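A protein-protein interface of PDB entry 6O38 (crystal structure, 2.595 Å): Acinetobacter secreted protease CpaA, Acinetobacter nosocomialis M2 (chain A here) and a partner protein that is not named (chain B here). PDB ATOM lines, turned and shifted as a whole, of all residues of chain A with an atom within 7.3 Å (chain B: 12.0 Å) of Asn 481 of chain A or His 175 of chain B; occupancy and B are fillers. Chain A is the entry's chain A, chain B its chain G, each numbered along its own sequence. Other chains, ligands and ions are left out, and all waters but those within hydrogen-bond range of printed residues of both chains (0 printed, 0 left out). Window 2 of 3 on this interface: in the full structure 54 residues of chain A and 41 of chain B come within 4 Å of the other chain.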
ATOM      1  N   ILE A 437     -19.601  25.238  20.363  1.00  0.00           N
ATOM      2  CA  ILE A 437     -20.910  25.785  20.702  1.00  0.00           C
ATOM      3  C   ILE A 437     -21.547  26.452  19.488  1.00  0.00           C
ATOM      4  O   ILE A 437     -22.777  26.559  19.405  1.00  0.00           O
ATOM      5  CB  ILE A 437     -20.792  26.754  21.895  1.00  0.00           C
ATOM      6  CG1 ILE A 437     -22.104  26.798  22.680  1.00  0.00           C
ATOM      7  CG2 ILE A 437     -20.389  28.148  21.434  1.00  0.00           C
ATOM      8  CD1 ILE A 437     -22.436  25.491  23.355  1.00  0.00           C
ATOM      9  N   SER A 438     -20.734  26.912  18.536  1.00  0.00           N
ATOM     10  CA  SER A 438     -21.259  27.529  17.323  1.00  0.00           C
ATOM     11  C   SER A 438     -21.728  26.476  16.326  1.00  0.00           C
ATOM     12  O   SER A 438     -22.904  26.440  15.950  1.00  0.00           O
ATOM     13  CB  SER A 438     -20.195  28.434  16.695  1.00  0.00           C
ATOM     14  OG  SER A 438     -20.235  29.733  17.256  1.00  0.00           O
ATOM     15  N   ARG A 441     -24.883  24.054  16.633  1.00  0.00           N
ATOM     16  CA  ARG A 441     -26.242  24.488  16.328  1.00  0.00           C
ATOM     17  C   ARG A 441     -26.688  24.013  14.952  1.00  0.00           C
ATOM     18  O   ARG A 441     -27.890  23.866  14.707  1.00  0.00           O
ATOM     19  CB  ARG A 441     -26.330  26.010  16.417  1.00  0.00           C
ATOM     20  CG  ARG A 441     -25.814  26.583  17.725  1.00  0.00           C
ATOM     21  CD  ARG A 441     -25.733  28.098  17.663  1.00  0.00           C
ATOM     22  NE  ARG A 441     -24.888  28.549  16.559  1.00  0.00           N
ATOM     23  CZ  ARG A 441     -24.582  29.820  16.322  1.00  0.00           C
ATOM     24  NH1 ARG A 441     -25.056  30.776  17.110  1.00  0.00           N
ATOM     25  NH2 ARG A 441     -23.804  30.138  15.297  1.00  0.00           N
ATOM     26  N   ARG A 450     -31.857  15.744  17.984  1.00  0.00           N
ATOM     27  CA  ARG A 450     -32.650  16.690  18.761  1.00  0.00           C
ATOM     28  C   ARG A 450     -34.103  16.692  18.301  1.00  0.00           C
ATOM     29  O   ARG A 450     -35.025  16.680  19.126  1.00  0.00           O
ATOM     30  CB  ARG A 450     -32.048  18.091  18.650  1.00  0.00           C
ATOM     31  CG  ARG A 450     -32.774  19.154  19.458  1.00  0.00           C
ATOM     32  CD  ARG A 450     -32.333  20.549  19.044  1.00  0.00           C
ATOM     33  NE  ARG A 450     -33.007  21.592  19.811  1.00  0.00           N
ATOM     34  CZ  ARG A 450     -32.821  22.895  19.625  1.00  0.00           C
ATOM     35  NH1 ARG A 450     -31.978  23.320  18.693  1.00  0.00           N
ATOM     36  NH2 ARG A 450     -33.477  23.773  20.371  1.00  0.00           N
ATOM     37  N   VAL A 458     -29.922  21.232  23.862  1.00  0.00           N
ATOM     38  CA  VAL A 458     -28.812  20.301  23.703  1.00  0.00           C
ATOM     39  C   VAL A 458     -27.669  20.763  24.596  1.00  0.00           C
ATOM     40  O   VAL A 458     -27.424  21.966  24.736  1.00  0.00           O
ATOM     41  CB  VAL A 458     -28.368  20.195  22.225  1.00  0.00           C
ATOM     42  CG1 VAL A 458     -28.233  21.574  21.605  1.00  0.00           C
ATOM     43  CG2 VAL A 458     -27.065  19.413  22.096  1.00  0.00           C
ATOM     44  N   ALA A 473     -21.995  28.964  26.631  1.00  0.00           N
ATOM     45  CA  ALA A 473     -23.437  28.902  26.423  1.00  0.00           C
ATOM     46  C   ALA A 473     -23.972  30.245  25.940  1.00  0.00           C
ATOM     47  O   ALA A 473     -23.618  31.293  26.491  1.00  0.00           O
ATOM     48  CB  ALA A 473     -24.157  28.482  27.707  1.00  0.00           C
ATOM     49  N   TRP A 474     -24.816  30.225  24.912  1.00  0.00           N
ATOM     50  CA  TRP A 474     -25.436  31.451  24.428  1.00  0.00           C
ATOM     51  C   TRP A 474     -26.404  32.008  25.465  1.00  0.00           C
ATOM     52  O   TRP A 474     -27.181  31.269  26.074  1.00  0.00           O
ATOM     53  CB  TRP A 474     -26.165  31.190  23.110  1.00  0.00           C
ATOM     54  CG  TRP A 474     -25.280  30.629  22.040  1.00  0.00           C
ATOM     55  CD1 TRP A 474     -25.188  29.324  21.654  1.00  0.00           C
ATOM     56  CD2 TRP A 474     -24.368  31.358  21.208  1.00  0.00           C
ATOM     57  NE1 TRP A 474     -24.269  29.193  20.640  1.00  0.00           N
ATOM     58  CE2 TRP A 474     -23.752  30.428  20.347  1.00  0.00           C
ATOM     59  CE3 TRP A 474     -24.010  32.707  21.111  1.00  0.00           C
ATOM     60  CZ2 TRP A 474     -22.799  30.802  19.401  1.00  0.00           C
ATOM     61  CZ3 TRP A 474     -23.063  33.076  20.172  1.00  0.00           C
ATOM     62  CH2 TRP A 474     -22.469  32.127  19.329  1.00  0.00           C
ATOM     63  N   ILE A 475     -26.354  33.323  25.663  1.00  0.00           N
ATOM     64  CA  ILE A 475     -27.180  33.998  26.658  1.00  0.00           C
ATOM     65  C   ILE A 475     -28.527  34.342  26.038  1.00  0.00           C
ATOM     66  O   ILE A 475     -28.588  34.902  24.936  1.00  0.00           O
ATOM     67  CB  ILE A 475     -26.479  35.257  27.193  1.00  0.00           C
ATOM     68  CG1 ILE A 475     -25.126  34.889  27.805  1.00  0.00           C
ATOM     69  CG2 ILE A 475     -27.360  35.959  28.214  1.00  0.00           C
ATOM     70  CD1 ILE A 475     -24.499  35.997  28.620  1.00  0.00           C
ATOM     71  N   ASN A 476     -29.608  34.009  26.748  1.00  0.00           N
ATOM     72  CA  ASN A 476     -30.976  34.282  26.305  1.00  0.00           C
ATOM     73  C   ASN A 476     -31.223  33.646  24.935  1.00  0.00           C
ATOM     74  O   ASN A 476     -31.593  34.304  23.960  1.00  0.00           O
ATOM     75  CB  ASN A 476     -31.258  35.789  26.285  1.00  0.00           C
ATOM     76  CG  ASN A 476     -32.736  36.105  26.170  1.00  0.00           C
ATOM     77  OD1 ASN A 476     -33.584  35.347  26.640  1.00  0.00           O
ATOM     78  ND2 ASN A 476     -33.053  37.233  25.543  1.00  0.00           N
ATOM     79  N   ALA A 477     -31.014  32.335  24.888  1.00  0.00           N
ATOM     80  CA  ALA A 477     -30.906  31.622  23.624  1.00  0.00           C
ATOM     81  C   ALA A 477     -32.276  31.377  23.009  1.00  0.00           C
ATOM     82  O   ALA A 477     -33.216  30.968  23.698  1.00  0.00           O
ATOM     83  CB  ALA A 477     -30.181  30.294  23.833  1.00  0.00           C
ATOM     84  N   SER A 478     -32.385  31.633  21.708  1.00  0.00           N
ATOM     85  CA  SER A 478     -33.528  31.176  20.936  1.00  0.00           C
ATOM     86  C   SER A 478     -33.453  29.660  20.755  1.00  0.00           C
ATOM     87  O   SER A 478     -32.525  28.995  21.223  1.00  0.00           O
ATOM     88  CB  SER A 478     -33.575  31.889  19.586  1.00  0.00           C
ATOM     89  OG  SER A 478     -32.424  31.597  18.815  1.00  0.00           O
ATOM     90  N   ALA A 479     -34.458  29.106  20.073  1.00  0.00           N
ATOM     91  CA  ALA A 479     -34.438  27.678  19.769  1.00  0.00           C
ATOM     92  C   ALA A 479     -33.188  27.298  18.984  1.00  0.00           C
ATOM     93  O   ALA A 479     -32.633  26.209  19.173  1.00  0.00           O
ATOM     94  CB  ALA A 479     -35.698  27.286  18.998  1.00  0.00           C
ATOM     95  N   TYR A 480     -32.728  28.187  18.100  1.00  0.00           N
ATOM     96  CA  TYR A 480     -31.527  27.909  17.322  1.00  0.00           C
ATOM     97  C   TYR A 480     -30.268  27.924  18.182  1.00  0.00           C
ATOM     98  O   TYR A 480     -29.330  27.164  17.915  1.00  0.00           O
ATOM     99  CB  TYR A 480     -31.400  28.918  16.181  1.00  0.00           C
ATOM    100  CG  TYR A 480     -30.113  28.796  15.399  1.00  0.00           C
ATOM    101  CD1 TYR A 480     -29.911  27.742  14.518  1.00  0.00           C
ATOM    102  CD2 TYR A 480     -29.101  29.737  15.541  1.00  0.00           C
ATOM    103  CE1 TYR A 480     -28.735  27.627  13.802  1.00  0.00           C
ATOM    104  CE2 TYR A 480     -27.922  29.629  14.828  1.00  0.00           C
ATOM    105  CZ  TYR A 480     -27.745  28.573  13.961  1.00  0.00           C
ATOM    106  OH  TYR A 480     -26.572  28.463  13.249  1.00  0.00           O
ATOM    107  N   ASN A 481     -30.226  28.768  19.212  1.00  0.00           N
ATOM    108  CA  ASN A 481     -29.035  28.940  20.033  1.00  0.00           C
ATOM    109  C   ASN A 481     -29.102  28.174  21.347  1.00  0.00           C
ATOM    110  O   ASN A 481     -28.212  28.332  22.189  1.00  0.00           O
ATOM    111  CB  ASN A 481     -28.799  30.426  20.315  1.00  0.00           C
ATOM    112  CG  ASN A 481     -28.336  31.185  19.090  1.00  0.00           C
ATOM    113  OD1 ASN A 481     -27.401  30.771  18.405  1.00  0.00           O
ATOM    114  ND2 ASN A 481     -28.986  32.309  18.809  1.00  0.00           N
ATOM    115  N   MET A 482     -30.122  27.345  21.540  1.00  0.00           N
ATOM    116  CA  MET A 482     -30.283  26.623  22.795  1.00  0.00           C
ATOM    117  C   MET A 482     -29.271  25.487  22.900  1.00  0.00           C
ATOM    118  O   MET A 482     -29.599  24.327  22.649  1.00  0.00           O
ATOM    119  CB  MET A 482     -31.708  26.081  22.923  1.00  0.00           C
ATOM    120  CG  MET A 482     -32.047  25.548  24.304  1.00  0.00           C
ATOM    121  SD  MET A 482     -32.000  26.934  25.671  1.00  0.00           S
ATOM    122  CE  MET A 482     -32.117  25.798  27.252  1.00  0.00           C
ATOM    123  N   ILE A 483     -28.038  25.826  23.267  1.00  0.00           N
ATOM    124  CA  ILE A 483     -26.966  24.841  23.381  1.00  0.00           C
ATOM    125  C   ILE A 483     -25.976  25.319  24.436  1.00  0.00           C
ATOM    126  O   ILE A 483     -25.703  26.516  24.556  1.00  0.00           O
ATOM    127  CB  ILE A 483     -26.278  24.599  22.018  1.00  0.00           C
ATOM    128  CG1 ILE A 483     -25.207  23.512  22.132  1.00  0.00           C
ATOM    129  CG2 ILE A 483     -25.687  25.890  21.467  1.00  0.00           C
ATOM    130  CD1 ILE A 483     -24.616  23.096  20.804  1.00  0.00           C
ATOM    131  N   GLY A 484     -25.453  24.371  25.213  1.00  0.00           N
ATOM    132  CA  GLY A 484     -24.453  24.674  26.215  1.00  0.00           C
ATOM    133  C   GLY A 484     -23.400  23.585  26.247  1.00  0.00           C
ATOM    134  O   GLY A 484     -23.631  22.457  25.802  1.00  0.00           O
ATOM    135  N   ASN A 503     -28.233  30.108  29.156  1.00  0.00           N
ATOM    136  CA  ASN A 503     -29.259  29.806  28.160  1.00  0.00           C
ATOM    137  C   ASN A 503     -30.608  30.395  28.554  1.00  0.00           C
ATOM    138  O   ASN A 503     -31.370  30.853  27.695  1.00  0.00           O
ATOM    139  CB  ASN A 503     -29.376  28.294  27.969  1.00  0.00           C
ATOM    140  CG  ASN A 503     -28.228  27.715  27.165  1.00  0.00           C
ATOM    141  OD1 ASN A 503     -27.509  28.440  26.477  1.00  0.00           O
ATOM    142  ND2 ASN A 503     -28.054  26.401  27.243  1.00  0.00           N
ATOM    143  N   TYR A 571     -39.971  24.810  22.769  1.00  0.00           N
ATOM    144  CA  TYR A 571     -39.193  24.815  21.533  1.00  0.00           C
ATOM    145  C   TYR A 571     -39.492  23.577  20.695  1.00  0.00           C
ATOM    146  O   TYR A 571     -39.652  23.669  19.472  1.00  0.00           O
ATOM    147  CB  TYR A 571     -37.700  24.902  21.848  1.00  0.00           C
ATOM    148  CG  TYR A 571     -37.219  26.286  22.227  1.00  0.00           C
ATOM    149  CD1 TYR A 571     -38.000  27.407  21.982  1.00  0.00           C
ATOM    150  CD2 TYR A 571     -35.977  26.471  22.824  1.00  0.00           C
ATOM    151  CE1 TYR A 571     -37.561  28.675  22.326  1.00  0.00           C
ATOM    152  CE2 TYR A 571     -35.530  27.732  23.170  1.00  0.00           C
ATOM    153  CZ  TYR A 571     -36.325  28.830  22.918  1.00  0.00           C
ATOM    154  OH  TYR A 571     -35.881  30.087  23.263  1.00  0.00           O
ATOM    155  N   GLN B 171     -16.607  33.037  30.259  1.00  0.00           N
ATOM    156  CA  GLN B 171     -16.878  34.412  29.880  1.00  0.00           C
ATOM    157  C   GLN B 171     -18.228  34.492  29.180  1.00  0.00           C
ATOM    158  O   GLN B 171     -18.680  33.529  28.553  1.00  0.00           O
ATOM    159  CB  GLN B 171     -15.780  34.957  28.957  1.00  0.00           C
ATOM    160  CG  GLN B 171     -14.382  34.876  29.538  1.00  0.00           C
ATOM    161  CD  GLN B 171     -13.343  35.515  28.645  1.00  0.00           C
ATOM    162  OE1 GLN B 171     -12.434  34.848  28.153  1.00  0.00           O
ATOM    163  NE2 GLN B 171     -13.464  36.822  28.439  1.00  0.00           N
ATOM    164  N   GLU B 172     -18.880  35.645  29.307  1.00  0.00           N
ATOM    165  CA  GLU B 172     -20.131  35.872  28.597  1.00  0.00           C
ATOM    166  C   GLU B 172     -19.893  35.833  27.093  1.00  0.00           C
ATOM    167  O   GLU B 172     -18.929  36.411  26.583  1.00  0.00           O
ATOM    168  CB  GLU B 172     -20.742  37.213  29.008  1.00  0.00           C
ATOM    169  CG  GLU B 172     -21.255  37.241  30.438  1.00  0.00           C
ATOM    170  CD  GLU B 172     -21.859  38.578  30.816  1.00  0.00           C
ATOM    171  OE1 GLU B 172     -21.926  39.472  29.946  1.00  0.00           O
ATOM    172  OE2 GLU B 172     -22.274  38.735  31.985  1.00  0.00           O
ATOM    173  N   LEU B 173     -20.780  35.143  26.383  1.00  0.00           N
ATOM    174  CA  LEU B 173     -20.636  34.909  24.953  1.00  0.00           C
ATOM    175  C   LEU B 173     -21.540  35.874  24.195  1.00  0.00           C
ATOM    176  O   LEU B 173     -22.712  36.043  24.550  1.00  0.00           O
ATOM    177  CB  LEU B 173     -20.980  33.460  24.607  1.00  0.00           C
ATOM    178  CG  LEU B 173     -20.934  33.039  23.138  1.00  0.00           C
ATOM    179  CD1 LEU B 173     -19.558  33.303  22.552  1.00  0.00           C
ATOM    180  CD2 LEU B 173     -21.297  31.569  23.007  1.00  0.00           C
ATOM    181  N   HIS B 174     -20.993  36.504  23.160  1.00  0.00           N
ATOM    182  CA  HIS B 174     -21.704  37.514  22.391  1.00  0.00           C
ATOM    183  C   HIS B 174     -21.768  37.112  20.923  1.00  0.00           C
ATOM    184  O   HIS B 174     -21.117  36.162  20.481  1.00  0.00           O
ATOM    185  CB  HIS B 174     -21.015  38.879  22.525  1.00  0.00           C
ATOM    186  CG  HIS B 174     -20.793  39.309  23.941  1.00  0.00           C
ATOM    187  ND1 HIS B 174     -21.824  39.656  24.788  1.00  0.00           N
ATOM    188  CD2 HIS B 174     -19.654  39.446  24.661  1.00  0.00           C
ATOM    189  CE1 HIS B 174     -21.330  39.989  25.967  1.00  0.00           C
ATOM    190  NE2 HIS B 174     -20.016  39.869  25.917  1.00  0.00           N
ATOM    191  N   HIS B 175     -22.569  37.857  20.167  1.00  0.00           N
ATOM    192  CA  HIS B 175     -22.728  37.612  18.738  1.00  0.00           C
ATOM    193  C   HIS B 175     -21.708  38.415  17.936  1.00  0.00           C
ATOM    194  O   HIS B 175     -21.620  38.284  16.715  1.00  0.00           O
ATOM    195  CB  HIS B 175     -24.148  37.952  18.283  1.00  0.00           C
ATOM    196  CG  HIS B 175     -25.191  37.009  18.799  1.00  0.00           C
ATOM    197  ND1 HIS B 175     -25.531  35.846  18.142  1.00  0.00           N
ATOM    198  CD2 HIS B 175     -25.969  37.055  19.906  1.00  0.00           C
ATOM    199  CE1 HIS B 175     -26.472  35.216  18.821  1.00  0.00           C
ATOM    200  NE2 HIS B 175     -26.756  35.930  19.896  1.00  0.00           N
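The guanidinium group (NH1) of Arg 441 of chain A is in hydrogen-bond range of the side-chain amide oxygen (OD1) of Asn 481 of chain A (2.7 Å). The indole nitrogen (NE1) of Trp 474 of chain A is in hydrogen-bond range of the backbone carbonyl oxygen (O) of Ile 437 of chain A. The backbone carbonyl oxygen (O) of Trp 474 of chain A lies close to the side-chain amide oxygen (OD1) of Asn 503 of chain A (2.9 Å).
Among the printed residues, merely in contact across the chains: Trp 474 of chain A with Leu 173 of chain B (3.5 Å), Trp 474 of chain A with His 174 of chain B (3.7 Å), Asn 481 of chain A with His 175 of chain B (3.8 Å), Ile 437 of chain A with Leu 173 of chain B (3.9 Å), Ala 473 of chain A with Leu 173 of chain B (3.9 Å) and Ile 475 of chain A with Glu 172 of chain B (3.9 Å).
Ala 473 of chain A touches just one residue of chain B: Leu 173 (3.9 Å). Trp 474 of chain A touches just these residues of chain B: Leu 173 and His 174. No residue of chain B comes within 4 Å of Ala 477 of chain A. No residue of chain B comes within 4 Å of Ala 479 of chain A. Asn 481 of chain A touches just one residue of chain B: His 175 (3.8 Å). No residue of chain B comes within 4 Å of Met 482 of chain A. No residue of chain B comes within 4 Å of Ile 483 of chain A. No residue of chain B comes within 4 Å of Asn 503 of chain A. Tyr 571 of chain A touches none of the printed residues of chain B. Gln 171 of chain B touches none of the printed residues of chain A. Printed residues of chain A within 4 Å of Leu 173 of chain B: Ile 437, Ala 473 and Trp 474. Of the printed residues of chain A, His 174 of chain B touches Trp 474 (3.7 Å). His 175 of chain B touches just one residue of chain A: Asn 481 (3.8 Å). The nearest residue of chain A that does not touch His 175 of chain B is Trp 474 of chain A (4.2 Å).
Printed residues of chain A that touch a printed residue of chain B: Ile 437, Ala 473, Trp 474, Ile 475 and Asn 481. Hydrophobic or aromatic side chains of chain A that line the printed part of chain B: Ile 437, Trp 474 and Ile 475. Of the 5 printed residues of chain B, 4 touch a printed residue of chain A. Along chain B the printed residues that touch a printed residue of chain A span positions 172 to 175. Among the printed residues, 6 pairs touch across the chains.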
